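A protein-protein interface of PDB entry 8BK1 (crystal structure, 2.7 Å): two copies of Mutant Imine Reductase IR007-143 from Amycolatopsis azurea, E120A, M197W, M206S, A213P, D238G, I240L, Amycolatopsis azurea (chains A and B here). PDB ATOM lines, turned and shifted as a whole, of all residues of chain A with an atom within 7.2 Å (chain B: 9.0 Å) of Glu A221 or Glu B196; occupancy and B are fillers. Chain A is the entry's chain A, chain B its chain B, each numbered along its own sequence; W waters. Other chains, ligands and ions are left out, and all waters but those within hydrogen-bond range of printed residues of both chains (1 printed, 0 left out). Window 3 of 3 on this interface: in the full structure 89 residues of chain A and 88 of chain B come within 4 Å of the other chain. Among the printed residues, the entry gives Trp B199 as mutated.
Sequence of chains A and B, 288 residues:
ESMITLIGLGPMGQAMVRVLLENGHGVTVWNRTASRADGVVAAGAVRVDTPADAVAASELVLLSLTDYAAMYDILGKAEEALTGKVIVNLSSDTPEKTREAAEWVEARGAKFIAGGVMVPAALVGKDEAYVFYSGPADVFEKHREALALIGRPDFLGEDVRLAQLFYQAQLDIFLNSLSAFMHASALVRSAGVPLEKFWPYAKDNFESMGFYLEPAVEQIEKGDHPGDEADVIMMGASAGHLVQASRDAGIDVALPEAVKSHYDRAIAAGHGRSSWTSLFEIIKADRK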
ATOM      1  N   ALA A 216      24.910  29.464 -33.482  1.00  0.00           N
ATOM      2  CA  ALA A 216      23.854  28.690 -32.798  1.00  0.00           C
ATOM      3  C   ALA A 216      24.087  28.708 -31.294  1.00  0.00           C
ATOM      4  O   ALA A 216      23.125  28.468 -30.534  1.00  0.00           O
ATOM      5  CB  ALA A 216      23.832  27.272 -33.318  1.00  0.00           C
ATOM      6  N   VAL A 217      25.323  28.914 -30.858  1.00  0.00           N
ATOM      7  CA  VAL A 217      25.632  28.878 -29.392  1.00  0.00           C
ATOM      8  C   VAL A 217      24.801  29.945 -28.667  1.00  0.00           C
ATOM      9  O   VAL A 217      24.167  29.618 -27.670  1.00  0.00           O
ATOM     10  CB  VAL A 217      27.130  29.079 -29.134  1.00  0.00           C
ATOM     11  CG1 VAL A 217      27.447  29.200 -27.672  1.00  0.00           C
ATOM     12  CG2 VAL A 217      27.918  27.943 -29.740  1.00  0.00           C
ATOM     13  N   GLU A 218      24.822  31.176 -29.173  1.00  0.00           N
ATOM     14  CA  GLU A 218      24.081  32.312 -28.593  1.00  0.00           C
ATOM     15  C   GLU A 218      22.587  31.976 -28.592  1.00  0.00           C
ATOM     16  O   GLU A 218      21.954  32.117 -27.529  1.00  0.00           O
ATOM     17  CB  GLU A 218      24.363  33.549 -29.424  1.00  0.00           C
ATOM     18  CG  GLU A 218      24.266  34.859 -28.669  1.00  0.00           C
ATOM     19  CD  GLU A 218      24.169  36.033 -29.628  1.00  0.00           C
ATOM     20  OE1 GLU A 218      24.190  35.802 -30.864  1.00  0.00           O
ATOM     21  OE2 GLU A 218      24.084  37.163 -29.149  1.00  0.00           O
ATOM     22  N   GLN A 219      22.052  31.526 -29.734  1.00  0.00           N
ATOM     23  CA  GLN A 219      20.627  31.128 -29.835  1.00  0.00           C
ATOM     24  C   GLN A 219      20.274  30.109 -28.742  1.00  0.00           C
ATOM     25  O   GLN A 219      19.218  30.249 -28.100  1.00  0.00           O
ATOM     26  CB  GLN A 219      20.357  30.545 -31.213  1.00  0.00           C
ATOM     27  CG  GLN A 219      20.452  31.581 -32.319  1.00  0.00           C
ATOM     28  CD  GLN A 219      19.781  31.119 -33.593  1.00  0.00           C
ATOM     29  OE1 GLN A 219      19.105  30.074 -33.655  1.00  0.00           O
ATOM     30  NE2 GLN A 219      20.007  31.895 -34.640  1.00  0.00           N
ATOM     31  N   ILE A 220      21.131  29.117 -28.511  1.00  0.00           N
ATOM     32  CA  ILE A 220      20.826  28.055 -27.513  1.00  0.00           C
ATOM     33  C   ILE A 220      20.943  28.650 -26.107  1.00  0.00           C
ATOM     34  O   ILE A 220      20.087  28.329 -25.277  1.00  0.00           O
ATOM     35  CB  ILE A 220      21.711  26.814 -27.738  1.00  0.00           C
ATOM     36  CG1 ILE A 220      21.319  26.104 -29.033  1.00  0.00           C
ATOM     37  CG2 ILE A 220      21.644  25.851 -26.556  1.00  0.00           C
ATOM     38  CD1 ILE A 220      22.406  25.206 -29.590  1.00  0.00           C
ATOM     39  N   GLU A 221      21.967  29.457 -25.849  1.00  0.00           N
ATOM     40  CA  GLU A 221      22.174  30.113 -24.526  1.00  0.00           C
ATOM     41  C   GLU A 221      20.898  30.890 -24.158  1.00  0.00           C
ATOM     42  O   GLU A 221      20.461  30.751 -23.033  1.00  0.00           O
ATOM     43  CB  GLU A 221      23.394  31.053 -24.533  1.00  0.00           C
ATOM     44  CG  GLU A 221      24.724  30.356 -24.285  1.00  0.00           C
ATOM     45  CD  GLU A 221      25.992  31.145 -24.618  1.00  0.00           C
ATOM     46  OE1 GLU A 221      25.921  32.080 -25.467  1.00  0.00           O
ATOM     47  OE2 GLU A 221      27.089  30.771 -24.085  1.00  0.00           O
ATOM     48  N   LYS A 222      20.282  31.582 -25.113  1.00  0.00           N
ATOM     49  CA  LYS A 222      19.183  32.558 -24.906  1.00  0.00           C
ATOM     50  C   LYS A 222      17.771  31.993 -25.156  1.00  0.00           C
ATOM     51  O   LYS A 222      16.836  32.729 -24.862  1.00  0.00           O
ATOM     52  CB  LYS A 222      19.423  33.743 -25.838  1.00  0.00           C
ATOM     53  CG  LYS A 222      20.571  34.620 -25.370  1.00  0.00           C
ATOM     54  CD  LYS A 222      20.844  35.794 -26.265  1.00  0.00           C
ATOM     55  CE  LYS A 222      21.921  36.668 -25.653  1.00  0.00           C
ATOM     56  NZ  LYS A 222      22.607  37.490 -26.677  1.00  0.00           N
ATOM     57  N   GLY A 223      17.590  30.798 -25.732  1.00  0.00           N
ATOM     58  CA  GLY A 223      16.251  30.320 -26.128  1.00  0.00           C
ATOM     59  C   GLY A 223      15.662  31.150 -27.271  1.00  0.00           C
ATOM     60  O   GLY A 223      14.419  31.251 -27.356  1.00  0.00           O
ATOM     61  N   ASP A 224      16.512  31.645 -28.164  1.00  0.00           N
ATOM     62  CA  ASP A 224      16.167  32.611 -29.236  1.00  0.00           C
ATOM     63  C   ASP A 224      16.356  31.917 -30.592  1.00  0.00           C
ATOM     64  O   ASP A 224      17.511  31.826 -31.067  1.00  0.00           O
ATOM     65  CB  ASP A 224      17.054  33.855 -29.147  1.00  0.00           C
ATOM     66  CG  ASP A 224      16.379  35.087 -29.692  1.00  0.00           C
ATOM     67  OD1 ASP A 224      15.609  35.663 -28.932  1.00  0.00           O
ATOM     68  OD2 ASP A 224      16.613  35.446 -30.864  1.00  0.00           O
ATOM     69  N   HIS A 225      15.266  31.467 -31.202  1.00  0.00           N
ATOM     70  CA  HIS A 225      15.286  30.459 -32.280  1.00  0.00           C
ATOM     71  C   HIS A 225      14.575  30.993 -33.522  1.00  0.00           C
ATOM     72  O   HIS A 225      13.602  30.403 -33.979  1.00  0.00           O
ATOM     73  CB  HIS A 225      14.633  29.186 -31.759  1.00  0.00           C
ATOM     74  CG  HIS A 225      15.229  28.670 -30.492  1.00  0.00           C
ATOM     75  ND1 HIS A 225      16.561  28.291 -30.380  1.00  0.00           N
ATOM     76  CD2 HIS A 225      14.654  28.390 -29.307  1.00  0.00           C
ATOM     77  CE1 HIS A 225      16.775  27.831 -29.164  1.00  0.00           C
ATOM     78  NE2 HIS A 225      15.614  27.874 -28.485  1.00  0.00           N
ATOM     79  N   PHE A 280      16.963  22.020 -29.403  1.00  0.00           N
ATOM     80  CA  PHE A 280      17.559  22.048 -28.052  1.00  0.00           C
ATOM     81  C   PHE A 280      16.458  22.063 -26.971  1.00  0.00           C
ATOM     82  O   PHE A 280      16.632  21.403 -25.914  1.00  0.00           O
ATOM     83  CB  PHE A 280      18.520  23.222 -27.910  1.00  0.00           C
ATOM     84  CG  PHE A 280      19.277  23.163 -26.618  1.00  0.00           C
ATOM     85  CD1 PHE A 280      20.365  22.324 -26.493  1.00  0.00           C
ATOM     86  CD2 PHE A 280      18.881  23.905 -25.517  1.00  0.00           C
ATOM     87  CE1 PHE A 280      21.089  22.264 -25.314  1.00  0.00           C
ATOM     88  CE2 PHE A 280      19.598  23.833 -24.330  1.00  0.00           C
ATOM     89  CZ  PHE A 280      20.704  23.018 -24.232  1.00  0.00           C
ATOM     90  N   GLU A 281      15.344  22.752 -27.226  1.00  0.00           N
ATOM     91  CA  GLU A 281      14.247  22.910 -26.227  1.00  0.00           C
ATOM     92  C   GLU A 281      13.574  21.556 -25.943  1.00  0.00           C
ATOM     93  O   GLU A 281      13.147  21.386 -24.803  1.00  0.00           O
ATOM     94  CB  GLU A 281      13.214  23.937 -26.671  1.00  0.00           C
ATOM     95  CG  GLU A 281      13.782  25.342 -26.901  1.00  0.00           C
ATOM     96  CD  GLU A 281      14.407  26.018 -25.697  1.00  0.00           C
ATOM     97  OE1 GLU A 281      14.181  25.531 -24.567  1.00  0.00           O
ATOM     98  OE2 GLU A 281      15.135  27.026 -25.896  1.00  0.00           O
ATOM     99  N   LYS A 284      16.906  19.031 -24.311  1.00  0.00           N
ATOM    100  CA  LYS A 284      17.471  19.409 -22.980  1.00  0.00           C
ATOM    101  C   LYS A 284      16.652  18.746 -21.881  1.00  0.00           C
ATOM    102  O   LYS A 284      15.557  18.302 -22.160  1.00  0.00           O
ATOM    103  CB  LYS A 284      17.540  20.932 -22.814  1.00  0.00           C
ATOM    104  CG  LYS A 284      16.236  21.682 -22.563  1.00  0.00           C
ATOM    105  CD  LYS A 284      16.526  23.036 -21.941  1.00  0.00           C
ATOM    106  CE  LYS A 284      15.366  24.003 -21.988  1.00  0.00           C
ATOM    107  NZ  LYS A 284      15.852  25.399 -22.152  1.00  0.00           N
ATOM    108  N   PHE B 181      25.611  18.019 -31.855  1.00  0.00           N
ATOM    109  CA  PHE B 181      26.069  19.255 -31.182  1.00  0.00           C
ATOM    110  C   PHE B 181      25.082  19.609 -30.049  1.00  0.00           C
ATOM    111  O   PHE B 181      25.530  19.772 -28.882  1.00  0.00           O
ATOM    112  CB  PHE B 181      26.229  20.385 -32.179  1.00  0.00           C
ATOM    113  CG  PHE B 181      26.557  21.674 -31.488  1.00  0.00           C
ATOM    114  CD1 PHE B 181      27.739  21.776 -30.778  1.00  0.00           C
ATOM    115  CD2 PHE B 181      25.689  22.745 -31.507  1.00  0.00           C
ATOM    116  CE1 PHE B 181      28.082  22.943 -30.127  1.00  0.00           C
ATOM    117  CE2 PHE B 181      26.025  23.908 -30.841  1.00  0.00           C
ATOM    118  CZ  PHE B 181      27.213  23.999 -30.146  1.00  0.00           C
ATOM    119  N   SER B 185      25.778  19.421 -26.049  1.00  0.00           N
ATOM    120  CA  SER B 185      25.475  20.694 -25.354  1.00  0.00           C
ATOM    121  C   SER B 185      24.492  20.414 -24.210  1.00  0.00           C
ATOM    122  O   SER B 185      24.777  20.819 -23.054  1.00  0.00           O
ATOM    123  CB  SER B 185      24.957  21.718 -26.312  1.00  0.00           C
ATOM    124  OG  SER B 185      25.980  22.047 -27.237  1.00  0.00           O
ATOM    125  N   VAL B 188      26.023  18.619 -21.183  1.00  0.00           N
ATOM    126  CA  VAL B 188      26.878  19.600 -20.482  1.00  0.00           C
ATOM    127  C   VAL B 188      25.944  20.530 -19.694  1.00  0.00           C
ATOM    128  O   VAL B 188      26.174  20.636 -18.467  1.00  0.00           O
ATOM    129  CB  VAL B 188      27.755  20.326 -21.512  1.00  0.00           C
ATOM    130  CG1 VAL B 188      28.307  21.624 -20.984  1.00  0.00           C
ATOM    131  CG2 VAL B 188      28.870  19.422 -22.005  1.00  0.00           C
ATOM    132  N   ARG B 189      24.928  21.146 -20.340  1.00  0.00           N
ATOM    133  CA  ARG B 189      24.061  22.144 -19.656  1.00  0.00           C
ATOM    134  C   ARG B 189      23.319  21.412 -18.528  1.00  0.00           C
ATOM    135  O   ARG B 189      23.169  21.969 -17.449  1.00  0.00           O
ATOM    136  CB  ARG B 189      23.181  22.958 -20.613  1.00  0.00           C
ATOM    137  CG  ARG B 189      23.321  24.477 -20.412  1.00  0.00           C
ATOM    138  CD  ARG B 189      22.450  25.427 -21.260  1.00  0.00           C
ATOM    139  NE  ARG B 189      21.256  26.018 -20.622  1.00  0.00           N
ATOM    140  CZ  ARG B 189      20.141  25.354 -20.236  1.00  0.00           C
ATOM    141  NH1 ARG B 189      20.053  24.038 -20.354  1.00  0.00           N
ATOM    142  NH2 ARG B 189      19.127  25.990 -19.672  1.00  0.00           N
ATOM    143  N   VAL B 193      27.183  23.104 -16.360  1.00  0.00           N
ATOM    144  CA  VAL B 193      28.347  23.724 -17.048  1.00  0.00           C
ATOM    145  C   VAL B 193      27.813  24.599 -18.169  1.00  0.00           C
ATOM    146  O   VAL B 193      26.995  24.178 -18.960  1.00  0.00           O
ATOM    147  CB  VAL B 193      29.304  22.646 -17.583  1.00  0.00           C
ATOM    148  CG1 VAL B 193      30.463  23.252 -18.351  1.00  0.00           C
ATOM    149  CG2 VAL B 193      29.767  21.699 -16.488  1.00  0.00           C
ATOM    150  N   PRO B 194      28.212  25.881 -18.242  1.00  0.00           N
ATOM    151  CA  PRO B 194      27.799  26.731 -19.352  1.00  0.00           C
ATOM    152  C   PRO B 194      28.391  26.251 -20.689  1.00  0.00           C
ATOM    153  O   PRO B 194      29.522  25.820 -20.780  1.00  0.00           O
ATOM    154  CB  PRO B 194      28.334  28.120 -18.996  1.00  0.00           C
ATOM    155  CG  PRO B 194      29.428  27.868 -17.981  1.00  0.00           C
ATOM    156  CD  PRO B 194      29.041  26.590 -17.264  1.00  0.00           C
ATOM    157  N   LEU B 195      27.604  26.415 -21.727  1.00  0.00           N
ATOM    158  CA  LEU B 195      27.941  26.027 -23.101  1.00  0.00           C
ATOM    159  C   LEU B 195      29.210  26.740 -23.574  1.00  0.00           C
ATOM    160  O   LEU B 195      29.986  26.150 -24.323  1.00  0.00           O
ATOM    161  CB  LEU B 195      26.733  26.394 -23.947  1.00  0.00           C
ATOM    162  CG  LEU B 195      26.317  25.335 -24.937  1.00  0.00           C
ATOM    163  CD1 LEU B 195      24.814  25.105 -24.826  1.00  0.00           C
ATOM    164  CD2 LEU B 195      26.752  25.727 -26.337  1.00  0.00           C
ATOM    165  N   GLU B 196      29.444  27.974 -23.145  1.00  0.00           N
ATOM    166  CA  GLU B 196      30.633  28.754 -23.546  1.00  0.00           C
ATOM    167  C   GLU B 196      31.914  27.970 -23.180  1.00  0.00           C
ATOM    168  O   GLU B 196      32.873  28.036 -23.955  1.00  0.00           O
ATOM    169  CB  GLU B 196      30.519  30.133 -22.895  1.00  0.00           C
ATOM    170  CG  GLU B 196      31.526  31.115 -23.425  1.00  0.00           C
ATOM    171  CD  GLU B 196      32.131  32.002 -22.348  1.00  0.00           C
ATOM    172  OE1 GLU B 196      31.356  32.466 -21.463  1.00  0.00           O
ATOM    173  OE2 GLU B 196      33.382  32.169 -22.366  1.00  0.00           O
ATOM    174  N   LYS B 197      31.919  27.201 -22.084  1.00  0.00           N
ATOM    175  CA  LYS B 197      33.106  26.446 -21.599  1.00  0.00           C
ATOM    176  C   LYS B 197      33.368  25.250 -22.520  1.00  0.00           C
ATOM    177  O   LYS B 197      34.546  24.897 -22.673  1.00  0.00           O
ATOM    178  CB  LYS B 197      32.968  25.935 -20.155  1.00  0.00           C
ATOM    179  CG  LYS B 197      32.906  26.999 -19.068  1.00  0.00           C
ATOM    180  CD  LYS B 197      34.204  27.625 -18.652  1.00  0.00           C
ATOM    181  CE  LYS B 197      34.036  28.510 -17.431  1.00  0.00           C
ATOM    182  NZ  LYS B 197      35.243  29.338 -17.195  1.00  0.00           N
ATOM    183  N   PHE B 198      32.326  24.653 -23.109  1.00  0.00           N
ATOM    184  CA  PHE B 198      32.388  23.407 -23.912  1.00  0.00           C
ATOM    185  C   PHE B 198      32.608  23.719 -25.402  1.00  0.00           C
ATOM    186  O   PHE B 198      33.249  22.919 -26.084  1.00  0.00           O
ATOM    187  CB  PHE B 198      31.116  22.577 -23.709  1.00  0.00           C
ATOM    188  CG  PHE B 198      31.053  21.323 -24.551  1.00  0.00           C
ATOM    189  CD1 PHE B 198      31.955  20.283 -24.348  1.00  0.00           C
ATOM    190  CD2 PHE B 198      30.167  21.228 -25.616  1.00  0.00           C
ATOM    191  CE1 PHE B 198      31.928  19.156 -25.143  1.00  0.00           C
ATOM    192  CE2 PHE B 198      30.150  20.101 -26.418  1.00  0.00           C
ATOM    193  CZ  PHE B 198      31.029  19.071 -26.183  1.00  0.00           C
ATOM    194  N   TRP B 199      32.112  24.850 -25.899  1.00  0.00           N
ATOM    195  CA  TRP B 199      32.137  25.192 -27.345  1.00  0.00           C
ATOM    196  C   TRP B 199      33.529  25.016 -27.965  1.00  0.00           C
ATOM    197  O   TRP B 199      33.664  24.443 -29.044  1.00  0.00           O
ATOM    198  CB  TRP B 199      31.603  26.614 -27.567  1.00  0.00           C
ATOM    199  CG  TRP B 199      31.953  27.146 -28.918  1.00  0.00           C
ATOM    200  CD1 TRP B 199      32.822  28.158 -29.221  1.00  0.00           C
ATOM    201  CD2 TRP B 199      31.547  26.585 -30.170  1.00  0.00           C
ATOM    202  NE1 TRP B 199      32.945  28.289 -30.576  1.00  0.00           N
ATOM    203  CE2 TRP B 199      32.156  27.348 -31.185  1.00  0.00           C
ATOM    204  CE3 TRP B 199      30.702  25.535 -30.533  1.00  0.00           C
ATOM    205  CZ2 TRP B 199      31.943  27.092 -32.533  1.00  0.00           C
ATOM    206  CZ3 TRP B 199      30.448  25.319 -31.867  1.00  0.00           C
ATOM    207  CH2 TRP B 199      31.096  26.059 -32.852  1.00  0.00           C
ATOM    208  N   PRO B 200      34.618  25.538 -27.355  1.00  0.00           N
ATOM    209  CA  PRO B 200      35.940  25.436 -27.972  1.00  0.00           C
ATOM    210  C   PRO B 200      36.318  23.969 -28.241  1.00  0.00           C
ATOM    211  O   PRO B 200      36.906  23.685 -29.266  1.00  0.00           O
ATOM    212  CB  PRO B 200      36.900  26.112 -26.972  1.00  0.00           C
ATOM    213  CG  PRO B 200      36.017  26.897 -26.035  1.00  0.00           C
ATOM    214  CD  PRO B 200      34.663  26.209 -26.047  1.00  0.00           C
ATOM    215  N   TYR B 201      35.952  23.066 -27.342  1.00  0.00           N
ATOM    216  CA  TYR B 201      36.188  21.607 -27.488  1.00  0.00           C
ATOM    217  C   TYR B 201      35.315  21.048 -28.638  1.00  0.00           C
ATOM    218  O   TYR B 201      35.787  20.300 -29.518  1.00  0.00           O
ATOM    219  CB  TYR B 201      35.991  20.937 -26.135  1.00  0.00           C
ATOM    220  CG  TYR B 201      36.979  21.375 -25.080  1.00  0.00           C
ATOM    221  CD1 TYR B 201      38.285  20.916 -25.128  1.00  0.00           C
ATOM    222  CD2 TYR B 201      36.638  22.244 -24.036  1.00  0.00           C
ATOM    223  CE1 TYR B 201      39.212  21.259 -24.148  1.00  0.00           C
ATOM    224  CE2 TYR B 201      37.552  22.605 -23.046  1.00  0.00           C
ATOM    225  CZ  TYR B 201      38.847  22.118 -23.112  1.00  0.00           C
ATOM    226  OH  TYR B 201      39.750  22.369 -22.120  1.00  0.00           O
ATOM    227  N   ALA B 202      34.044  21.390 -28.679  1.00  0.00           N
ATOM    228  CA  ALA B 202      33.137  20.883 -29.726  1.00  0.00           C
ATOM    229  C   ALA B 202      33.672  21.348 -31.081  1.00  0.00           C
ATOM    230  O   ALA B 202      33.719  20.550 -32.035  1.00  0.00           O
ATOM    231  CB  ALA B 202      31.738  21.376 -29.458  1.00  0.00           C
HETATM  232  O   HOH W   1      18.178  26.822 -22.404  1.00  0.00           O
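OE1 of Glu A281 is in salt-bridge range of NZ of Lys A284, 2.9 Å away.
Among the printed residues, pairs that only touch across the chains: Glu A221 with Glu B196, Ile A220 with Leu B195, Val A217 with Trp B199, Val A217 with Leu B195 and Lys A284 with Arg B189.
Glu A218 touches none of the printed residues of chain B. Of chain B, only Glu B196 comes within 4 Å of Glu A221. Lys A222 touches none of the printed residues of chain B. Printed residues of chain B within 4 Å of Lys A284: Arg B189. Of the printed residues of chain A, Leu B195 touches Val A217 (3.8 Å) and Ile A220 (3.7 Å). Of chain A, only Glu A221 (3.7 Å) comes within 4 Å of Glu B196. Of the printed residues of chain A, Trp B199 touches Val A217. The nearest residue of chain B that does not touch Glu A221 is Leu B195 (4.4 Å). The nearest residue of chain A that does not touch Glu B196 is Val A217 (5.1 Å).
Printed residues of chain B that touch a printed residue of chain A: Arg B189, Leu B195, Glu B196 and Trp B199. Hydrophobic or aromatic side chains of chain B that line the printed part of chain A: Leu B195 and Trp B199. Of the 13 printed residues of chain A, 4 touch a printed residue of chain B. Among the printed residues, 5 pairs touch across the chains.
No position is printed for both chains. Of the 5 pairs that touch across the chains among the printed residues, none has its exchanged pair printed and touching as well.
Water W1 bridges the side-chain amino group of Lys A284 (2.7 Å) and the guanidinium group of Arg B189 (3.0 Å).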
